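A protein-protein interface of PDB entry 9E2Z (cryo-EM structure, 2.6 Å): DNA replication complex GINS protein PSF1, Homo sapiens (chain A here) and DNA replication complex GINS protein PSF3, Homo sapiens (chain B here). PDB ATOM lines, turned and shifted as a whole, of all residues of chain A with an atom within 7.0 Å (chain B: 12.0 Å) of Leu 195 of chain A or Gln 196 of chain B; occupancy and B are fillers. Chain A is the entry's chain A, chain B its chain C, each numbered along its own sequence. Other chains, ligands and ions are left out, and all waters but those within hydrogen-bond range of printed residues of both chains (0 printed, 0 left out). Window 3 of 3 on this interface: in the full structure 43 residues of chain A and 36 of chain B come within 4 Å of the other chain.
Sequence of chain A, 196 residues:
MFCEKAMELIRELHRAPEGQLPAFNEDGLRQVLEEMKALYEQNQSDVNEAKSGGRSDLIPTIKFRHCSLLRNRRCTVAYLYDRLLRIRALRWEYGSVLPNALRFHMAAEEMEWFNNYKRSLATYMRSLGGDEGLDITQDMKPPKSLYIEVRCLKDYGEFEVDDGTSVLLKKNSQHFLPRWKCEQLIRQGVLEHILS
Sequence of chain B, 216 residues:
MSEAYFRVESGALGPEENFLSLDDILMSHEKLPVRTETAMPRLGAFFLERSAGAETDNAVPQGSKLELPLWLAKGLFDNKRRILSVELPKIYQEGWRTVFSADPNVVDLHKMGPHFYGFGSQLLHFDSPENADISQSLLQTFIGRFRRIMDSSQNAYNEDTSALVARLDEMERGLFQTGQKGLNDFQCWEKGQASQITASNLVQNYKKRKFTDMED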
ATOM      1  N   LYS A 141      25.592 -12.475  24.735  1.00  0.00           N
ATOM      2  CA  LYS A 141      25.788 -11.328  23.867  1.00  0.00           C
ATOM      3  C   LYS A 141      25.464 -10.057  24.634  1.00  0.00           C
ATOM      4  O   LYS A 141      24.692 -10.093  25.595  1.00  0.00           O
ATOM      5  CB  LYS A 141      24.895 -11.411  22.623  1.00  0.00           C
ATOM      6  CG  LYS A 141      25.430 -12.318  21.537  1.00  0.00           C
ATOM      7  CD  LYS A 141      24.334 -12.719  20.557  1.00  0.00           C
ATOM      8  CE  LYS A 141      24.146 -11.689  19.451  1.00  0.00           C
ATOM      9  NZ  LYS A 141      22.993 -10.784  19.716  1.00  0.00           N
ATOM     10  N   ILE A 148      11.853  -8.379  24.116  1.00  0.00           N
ATOM     11  CA  ILE A 148      12.013  -8.767  22.723  1.00  0.00           C
ATOM     12  C   ILE A 148      10.772  -9.511  22.256  1.00  0.00           C
ATOM     13  O   ILE A 148       9.980 -10.020  23.054  1.00  0.00           O
ATOM     14  CB  ILE A 148      13.269  -9.638  22.496  1.00  0.00           C
ATOM     15  CG1 ILE A 148      13.215 -10.903  23.353  1.00  0.00           C
ATOM     16  CG2 ILE A 148      14.526  -8.844  22.800  1.00  0.00           C
ATOM     17  CD1 ILE A 148      14.272 -11.897  23.014  1.00  0.00           C
ATOM     18  N   GLU A 149      10.620  -9.577  20.939  1.00  0.00           N
ATOM     19  CA  GLU A 149       9.549 -10.322  20.293  1.00  0.00           C
ATOM     20  C   GLU A 149      10.089 -11.662  19.811  1.00  0.00           C
ATOM     21  O   GLU A 149      11.136 -11.717  19.161  1.00  0.00           O
ATOM     22  CB  GLU A 149       8.968  -9.528  19.122  1.00  0.00           C
ATOM     23  CG  GLU A 149       7.599 -10.006  18.676  1.00  0.00           C
ATOM     24  CD  GLU A 149       7.100  -9.287  17.440  1.00  0.00           C
ATOM     25  OE1 GLU A 149       7.931  -8.743  16.684  1.00  0.00           O
ATOM     26  OE2 GLU A 149       5.872  -9.273  17.218  1.00  0.00           O
ATOM     27  N   ILE A 186      15.930 -19.471  22.613  1.00  0.00           N
ATOM     28  CA  ILE A 186      16.395 -19.007  21.311  1.00  0.00           C
ATOM     29  C   ILE A 186      17.668 -19.741  20.914  1.00  0.00           C
ATOM     30  O   ILE A 186      17.822 -20.164  19.764  1.00  0.00           O
ATOM     31  CB  ILE A 186      16.602 -17.482  21.318  1.00  0.00           C
ATOM     32  CG1 ILE A 186      15.266 -16.764  21.506  1.00  0.00           C
ATOM     33  CG2 ILE A 186      17.261 -17.032  20.023  1.00  0.00           C
ATOM     34  CD1 ILE A 186      15.408 -15.310  21.861  1.00  0.00           C
ATOM     35  N   GLU A 192      12.480 -17.889  17.786  1.00  0.00           N
ATOM     36  CA  GLU A 192      13.190 -17.028  16.850  1.00  0.00           C
ATOM     37  C   GLU A 192      12.977 -15.580  17.259  1.00  0.00           C
ATOM     38  O   GLU A 192      11.858 -15.189  17.601  1.00  0.00           O
ATOM     39  CB  GLU A 192      12.710 -17.264  15.416  1.00  0.00           C
ATOM     40  CG  GLU A 192      13.090 -16.167  14.452  1.00  0.00           C
ATOM     41  CD  GLU A 192      13.033 -16.611  13.007  1.00  0.00           C
ATOM     42  OE1 GLU A 192      11.956 -16.491  12.387  1.00  0.00           O
ATOM     43  OE2 GLU A 192      14.068 -17.075  12.486  1.00  0.00           O
ATOM     44  N   HIS A 193      14.046 -14.793  17.224  1.00  0.00           N
ATOM     45  CA  HIS A 193      13.995 -13.394  17.631  1.00  0.00           C
ATOM     46  C   HIS A 193      13.570 -12.532  16.446  1.00  0.00           C
ATOM     47  O   HIS A 193      14.282 -12.462  15.440  1.00  0.00           O
ATOM     48  CB  HIS A 193      15.362 -12.960  18.157  1.00  0.00           C
ATOM     49  CG  HIS A 193      15.421 -11.532  18.597  1.00  0.00           C
ATOM     50  ND1 HIS A 193      16.610 -10.883  18.845  1.00  0.00           N
ATOM     51  CD2 HIS A 193      14.443 -10.628  18.835  1.00  0.00           C
ATOM     52  CE1 HIS A 193      16.362  -9.642  19.218  1.00  0.00           C
ATOM     53  NE2 HIS A 193      15.055  -9.460  19.217  1.00  0.00           N
ATOM     54  N   ILE A 194      12.420 -11.872  16.565  1.00  0.00           N
ATOM     55  CA  ILE A 194      11.867 -11.045  15.499  1.00  0.00           C
ATOM     56  C   ILE A 194      12.293  -9.603  15.722  1.00  0.00           C
ATOM     57  O   ILE A 194      12.014  -9.019  16.776  1.00  0.00           O
ATOM     58  CB  ILE A 194      10.334 -11.154  15.449  1.00  0.00           C
ATOM     59  CG1 ILE A 194       9.890 -12.614  15.330  1.00  0.00           C
ATOM     60  CG2 ILE A 194       9.784 -10.346  14.293  1.00  0.00           C
ATOM     61  CD1 ILE A 194      10.635 -13.406  14.282  1.00  0.00           C
ATOM     62  N   LEU A 195      12.957  -9.026  14.728  1.00  0.00           N
ATOM     63  CA  LEU A 195      13.309  -7.614  14.720  1.00  0.00           C
ATOM     64  C   LEU A 195      12.428  -6.892  13.713  1.00  0.00           C
ATOM     65  O   LEU A 195      12.273  -7.351  12.576  1.00  0.00           O
ATOM     66  CB  LEU A 195      14.786  -7.420  14.377  1.00  0.00           C
ATOM     67  CG  LEU A 195      15.765  -7.840  15.475  1.00  0.00           C
ATOM     68  CD1 LEU A 195      17.189  -7.826  14.959  1.00  0.00           C
ATOM     69  CD2 LEU A 195      15.632  -6.927  16.682  1.00  0.00           C
ATOM     70  N   SER A 196      11.842  -5.778  14.134  1.00  0.00           N
ATOM     71  CA  SER A 196      10.972  -4.998  13.262  1.00  0.00           C
ATOM     72  C   SER A 196      11.469  -3.563  13.142  1.00  0.00           C
ATOM     73  O   SER A 196      12.281  -3.250  12.274  1.00  0.00           O
ATOM     74  CB  SER A 196       9.536  -5.017  13.786  1.00  0.00           C
ATOM     75  OG  SER A 196       8.920  -6.265  13.526  1.00  0.00           O
ATOM     76  N   ASP B 185      32.428 -10.018  10.022  1.00  0.00           N
ATOM     77  CA  ASP B 185      31.871  -9.468  11.254  1.00  0.00           C
ATOM     78  C   ASP B 185      31.533  -7.990  11.094  1.00  0.00           C
ATOM     79  O   ASP B 185      30.458  -7.545  11.510  1.00  0.00           O
ATOM     80  CB  ASP B 185      32.849  -9.673  12.409  1.00  0.00           C
ATOM     81  CG  ASP B 185      32.216  -9.413  13.769  1.00  0.00           C
ATOM     82  OD1 ASP B 185      31.179 -10.036  14.074  1.00  0.00           O
ATOM     83  OD2 ASP B 185      32.756  -8.587  14.534  1.00  0.00           O
ATOM     84  N   GLN B 187      30.920  -6.333   8.293  1.00  0.00           N
ATOM     85  CA  GLN B 187      29.813  -6.178   7.356  1.00  0.00           C
ATOM     86  C   GLN B 187      28.481  -6.487   8.026  1.00  0.00           C
ATOM     87  O   GLN B 187      27.483  -5.802   7.783  1.00  0.00           O
ATOM     88  CB  GLN B 187      30.023  -7.080   6.140  1.00  0.00           C
ATOM     89  CG  GLN B 187      31.174  -6.656   5.240  1.00  0.00           C
ATOM     90  CD  GLN B 187      31.049  -5.227   4.752  1.00  0.00           C
ATOM     91  OE1 GLN B 187      31.976  -4.432   4.881  1.00  0.00           O
ATOM     92  NE2 GLN B 187      29.896  -4.895   4.184  1.00  0.00           N
ATOM     93  N   CYS B 188      28.443  -7.524   8.864  1.00  0.00           N
ATOM     94  CA  CYS B 188      27.218  -7.839   9.589  1.00  0.00           C
ATOM     95  C   CYS B 188      26.842  -6.717  10.547  1.00  0.00           C
ATOM     96  O   CYS B 188      25.668  -6.350  10.651  1.00  0.00           O
ATOM     97  CB  CYS B 188      27.384  -9.157  10.345  1.00  0.00           C
ATOM     98  SG  CYS B 188      27.324 -10.622   9.293  1.00  0.00           S
ATOM     99  N   TRP B 189      27.825  -6.161  11.255  1.00  0.00           N
ATOM    100  CA  TRP B 189      27.537  -5.081  12.194  1.00  0.00           C
ATOM    101  C   TRP B 189      26.989  -3.858  11.476  1.00  0.00           C
ATOM    102  O   TRP B 189      26.034  -3.231  11.944  1.00  0.00           O
ATOM    103  CB  TRP B 189      28.798  -4.717  12.976  1.00  0.00           C
ATOM    104  CG  TRP B 189      28.616  -3.538  13.880  1.00  0.00           C
ATOM    105  CD1 TRP B 189      27.981  -3.523  15.081  1.00  0.00           C
ATOM    106  CD2 TRP B 189      29.067  -2.200  13.648  1.00  0.00           C
ATOM    107  NE1 TRP B 189      28.006  -2.263  15.615  1.00  0.00           N
ATOM    108  CE2 TRP B 189      28.667  -1.429  14.754  1.00  0.00           C
ATOM    109  CE3 TRP B 189      29.771  -1.578  12.614  1.00  0.00           C
ATOM    110  CZ2 TRP B 189      28.947  -0.070  14.858  1.00  0.00           C
ATOM    111  CZ3 TRP B 189      30.045  -0.228  12.716  1.00  0.00           C
ATOM    112  CH2 TRP B 189      29.636   0.510  13.830  1.00  0.00           C
ATOM    113  N   GLU B 190      27.585  -3.497  10.340  1.00  0.00           N
ATOM    114  CA  GLU B 190      27.171  -2.285   9.644  1.00  0.00           C
ATOM    115  C   GLU B 190      25.775  -2.436   9.052  1.00  0.00           C
ATOM    116  O   GLU B 190      25.021  -1.462   8.974  1.00  0.00           O
ATOM    117  CB  GLU B 190      28.188  -1.939   8.559  1.00  0.00           C
ATOM    118  CG  GLU B 190      28.272  -0.458   8.250  1.00  0.00           C
ATOM    119  CD  GLU B 190      28.719  -0.170   6.832  1.00  0.00           C
ATOM    120  OE1 GLU B 190      28.346  -0.933   5.916  1.00  0.00           O
ATOM    121  OE2 GLU B 190      29.447   0.823   6.634  1.00  0.00           O
ATOM    122  N   LYS B 191      25.411  -3.647   8.640  1.00  0.00           N
ATOM    123  CA  LYS B 191      24.097  -3.910   8.073  1.00  0.00           C
ATOM    124  C   LYS B 191      23.026  -4.131   9.133  1.00  0.00           C
ATOM    125  O   LYS B 191      21.861  -4.319   8.778  1.00  0.00           O
ATOM    126  CB  LYS B 191      24.164  -5.128   7.152  1.00  0.00           C
ATOM    127  CG  LYS B 191      24.638  -4.811   5.746  1.00  0.00           C
ATOM    128  CD  LYS B 191      25.010  -6.075   4.980  1.00  0.00           C
ATOM    129  CE  LYS B 191      26.398  -6.002   4.362  1.00  0.00           C
ATOM    130  NZ  LYS B 191      26.340  -5.788   2.893  1.00  0.00           N
ATOM    131  N   GLY B 192      23.388  -4.117  10.414  1.00  0.00           N
ATOM    132  CA  GLY B 192      22.414  -4.265  11.474  1.00  0.00           C
ATOM    133  C   GLY B 192      22.026  -5.685  11.799  1.00  0.00           C
ATOM    134  O   GLY B 192      21.004  -5.898  12.456  1.00  0.00           O
ATOM    135  N   GLN B 193      22.804  -6.665  11.355  1.00  0.00           N
ATOM    136  CA  GLN B 193      22.510  -8.064  11.620  1.00  0.00           C
ATOM    137  C   GLN B 193      23.203  -8.592  12.869  1.00  0.00           C
ATOM    138  O   GLN B 193      22.945  -9.732  13.263  1.00  0.00           O
ATOM    139  CB  GLN B 193      22.911  -8.919  10.415  1.00  0.00           C
ATOM    140  CG  GLN B 193      22.454  -8.354   9.080  1.00  0.00           C
ATOM    141  CD  GLN B 193      23.118  -9.027   7.899  1.00  0.00           C
ATOM    142  OE1 GLN B 193      24.121  -9.718   8.048  1.00  0.00           O
ATOM    143  NE2 GLN B 193      22.560  -8.824   6.714  1.00  0.00           N
ATOM    144  N   ALA B 194      24.057  -7.794  13.505  1.00  0.00           N
ATOM    145  CA  ALA B 194      24.840  -8.260  14.640  1.00  0.00           C
ATOM    146  C   ALA B 194      24.084  -8.199  15.959  1.00  0.00           C
ATOM    147  O   ALA B 194      24.618  -8.653  16.975  1.00  0.00           O
ATOM    148  CB  ALA B 194      26.126  -7.438  14.758  1.00  0.00           C
ATOM    149  N   SER B 195      22.867  -7.660  15.973  1.00  0.00           N
ATOM    150  CA  SER B 195      22.111  -7.507  17.207  1.00  0.00           C
ATOM    151  C   SER B 195      21.075  -8.600  17.429  1.00  0.00           C
ATOM    152  O   SER B 195      20.618  -8.771  18.563  1.00  0.00           O
ATOM    153  CB  SER B 195      21.410  -6.145  17.226  1.00  0.00           C
ATOM    154  OG  SER B 195      20.740  -5.906  16.003  1.00  0.00           O
ATOM    155  N   GLN B 196      20.694  -9.340  16.393  1.00  0.00           N
ATOM    156  CA  GLN B 196      19.712 -10.402  16.567  1.00  0.00           C
ATOM    157  C   GLN B 196      20.316 -11.561  17.348  1.00  0.00           C
ATOM    158  O   GLN B 196      21.447 -11.980  17.085  1.00  0.00           O
ATOM    159  CB  GLN B 196      19.206 -10.891  15.214  1.00  0.00           C
ATOM    160  CG  GLN B 196      17.928 -11.698  15.308  1.00  0.00           C
ATOM    161  CD  GLN B 196      17.706 -12.599  14.115  1.00  0.00           C
ATOM    162  OE1 GLN B 196      18.567 -12.724  13.248  1.00  0.00           O
ATOM    163  NE2 GLN B 196      16.551 -13.244  14.071  1.00  0.00           N
ATOM    164  N   ILE B 197      19.559 -12.076  18.311  1.00  0.00           N
ATOM    165  CA  ILE B 197      19.943 -13.284  19.033  1.00  0.00           C
ATOM    166  C   ILE B 197      19.562 -14.486  18.182  1.00  0.00           C
ATOM    167  O   ILE B 197      18.414 -14.608  17.741  1.00  0.00           O
ATOM    168  CB  ILE B 197      19.263 -13.342  20.410  1.00  0.00           C
ATOM    169  CG1 ILE B 197      19.419 -12.014  21.156  1.00  0.00           C
ATOM    170  CG2 ILE B 197      19.845 -14.469  21.236  1.00  0.00           C
ATOM    171  CD1 ILE B 197      18.547 -11.903  22.370  1.00  0.00           C
ATOM    172  N   THR B 198      20.520 -15.378  17.949  1.00  0.00           N
ATOM    173  CA  THR B 198      20.347 -16.466  17.001  1.00  0.00           C
ATOM    174  C   THR B 198      20.668 -17.797  17.660  1.00  0.00           C
ATOM    175  O   THR B 198      21.304 -17.858  18.713  1.00  0.00           O
ATOM    176  CB  THR B 198      21.239 -16.283  15.768  1.00  0.00           C
ATOM    177  OG1 THR B 198      22.596 -16.092  16.184  1.00  0.00           O
ATOM    178  CG2 THR B 198      20.788 -15.084  14.956  1.00  0.00           C
ATOM    179  N   ALA B 199      20.212 -18.867  17.018  1.00  0.00           N
ATOM    180  CA  ALA B 199      20.560 -20.206  17.465  1.00  0.00           C
ATOM    181  C   ALA B 199      22.066 -20.408  17.384  1.00  0.00           C
ATOM    182  O   ALA B 199      22.739 -19.887  16.492  1.00  0.00           O
ATOM    183  CB  ALA B 199      19.841 -21.255  16.619  1.00  0.00           C
ATOM    184  N   SER B 200      22.597 -21.167  18.336  1.00  0.00           N
ATOM    185  CA  SER B 200      24.032 -21.388  18.394  1.00  0.00           C
ATOM    186  C   SER B 200      24.530 -22.041  17.107  1.00  0.00           C
ATOM    187  O   SER B 200      23.774 -22.661  16.356  1.00  0.00           O
ATOM    188  CB  SER B 200      24.388 -22.262  19.593  1.00  0.00           C
ATOM    189  OG  SER B 200      23.494 -23.351  19.708  1.00  0.00           O
ATOM    190  N   ASN B 201      25.832 -21.890  16.859  1.00  0.00           N
ATOM    191  CA  ASN B 201      26.425 -22.447  15.647  1.00  0.00           C
ATOM    192  C   ASN B 201      26.251 -23.959  15.596  1.00  0.00           C
ATOM    193  O   ASN B 201      25.851 -24.514  14.567  1.00  0.00           O
ATOM    194  CB  ASN B 201      27.905 -22.074  15.573  1.00  0.00           C
ATOM    195  CG  ASN B 201      28.137 -20.734  14.909  1.00  0.00           C
ATOM    196  OD1 ASN B 201      27.488 -20.398  13.920  1.00  0.00           O
ATOM    197  ND2 ASN B 201      29.070 -19.959  15.450  1.00  0.00           N
ATOM    198  N   GLN B 204      22.723 -24.952  14.765  1.00  0.00           N
ATOM    199  CA  GLN B 204      22.428 -24.772  13.348  1.00  0.00           C
ATOM    200  C   GLN B 204      22.996 -25.917  12.517  1.00  0.00           C
ATOM    201  O   GLN B 204      22.318 -26.443  11.627  1.00  0.00           O
ATOM    202  CB  GLN B 204      22.986 -23.436  12.867  1.00  0.00           C
ATOM    203  CG  GLN B 204      22.276 -22.223  13.443  1.00  0.00           C
ATOM    204  CD  GLN B 204      23.115 -20.964  13.349  1.00  0.00           C
ATOM    205  OE1 GLN B 204      24.249 -20.996  12.873  1.00  0.00           O
ATOM    206  NE2 GLN B 204      22.562 -19.849  13.805  1.00  0.00           N
ATOM    207  N   LYS B 208      19.889 -28.286  11.261  1.00  0.00           N
ATOM    208  CA  LYS B 208      19.588 -27.732   9.946  1.00  0.00           C
ATOM    209  C   LYS B 208      20.686 -28.075   8.951  1.00  0.00           C
ATOM    210  O   LYS B 208      21.027 -27.279   8.072  1.00  0.00           O
ATOM    211  CB  LYS B 208      19.381 -26.222  10.029  1.00  0.00           C
ATOM    212  CG  LYS B 208      18.243 -25.816  10.955  1.00  0.00           C
ATOM    213  CD  LYS B 208      17.813 -24.376  10.728  1.00  0.00           C
ATOM    214  CE  LYS B 208      16.563 -24.041  11.526  1.00  0.00           C
ATOM    215  NZ  LYS B 208      16.071 -22.661  11.257  1.00  0.00           N
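Among the printed residues, merely in contact across the chains: Lys 141 of chain A with Ala 194 of chain B (3.8 Å), Lys 141 of chain A with Ile 197 of chain B (3.9 Å), Ile 186 of chain A with Ile 197 of chain B (3.5 Å), Ile 186 of chain A with Ala 199 of chain B (3.6 Å) and Leu 195 of chain A with Gln 196 of chain B (3.7 Å).
The backbone carbonyl oxygen (O) of Ser 195 of chain B sits at hydrogen-bond distance from the side-chain amino group (NZ) of Lys 141 of chain A. The backbone carbonyl oxygen of Gln 196 of chain B sits at hydrogen-bond distance from the side-chain amino group of Lys 141 of chain A, 3.3 Å away. The backbone carbonyl oxygen of His 193 of chain A lies within hydrogen-bond range of the side-chain amide nitrogen of Gln 196 of chain B (2.8 Å). ND1 of His 193 of chain A is in hydrogen-bond range of N of Ile 197 of chain B (3.2 Å).
The backbone carbonyl oxygen of Ala 199 of chain B sits at hydrogen-bond distance from the side-chain amide nitrogen of Gln 204 of chain B (2.7 Å).
Leu 195 of chain A touches one residue of chain B. Of the printed residues of chain A, Gln 196 of chain B touches Lys 141 (3.3 Å), His 193 (2.8 Å) and Leu 195 (3.7 Å). Of the printed residues of chain B, His 193 of chain A touches Gln 196 and Ile 197. Of the printed residues of chain A, Ile 197 of chain B touches Lys 141, Ile 186 and His 193. Of the printed residues of chain A, Ala 199 of chain B touches Ile 186. Printed residues of chain B within 4 Å of Lys 141 of chain A: Ala 194 (3.8 Å), Ser 195 (3.3 Å), Gln 196 (3.3 Å) and Ile 197 (3.9 Å). Printed residues of chain B within 4 Å of Ile 186 of chain A: Ile 197 (3.5 Å) and Ala 199 (3.6 Å). Gln 193 of chain B touches none of the printed residues of chain A. Thr 198 of chain B touches none of the printed residues of chain A. The nearest residue of chain B that does not touch Leu 195 of chain A is Ser 195 of chain B (4.2 Å). The nearest residue of chain A that does not touch Gln 196 of chain B is Glu 192 of chain A (4.5 Å).
Of the 18 printed residues of chain B, 5 touch a printed residue of chain A. Hydrophobic or aromatic side chains of chain B that line the printed part of chain A: Ile 197 and Ala 199. Of the 9 printed residues of chain A, 4 touch a printed residue of chain B. Printed residues of chain A that touch a printed residue of chain B: Lys 141, Ile 186, His 193 and Leu 195.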
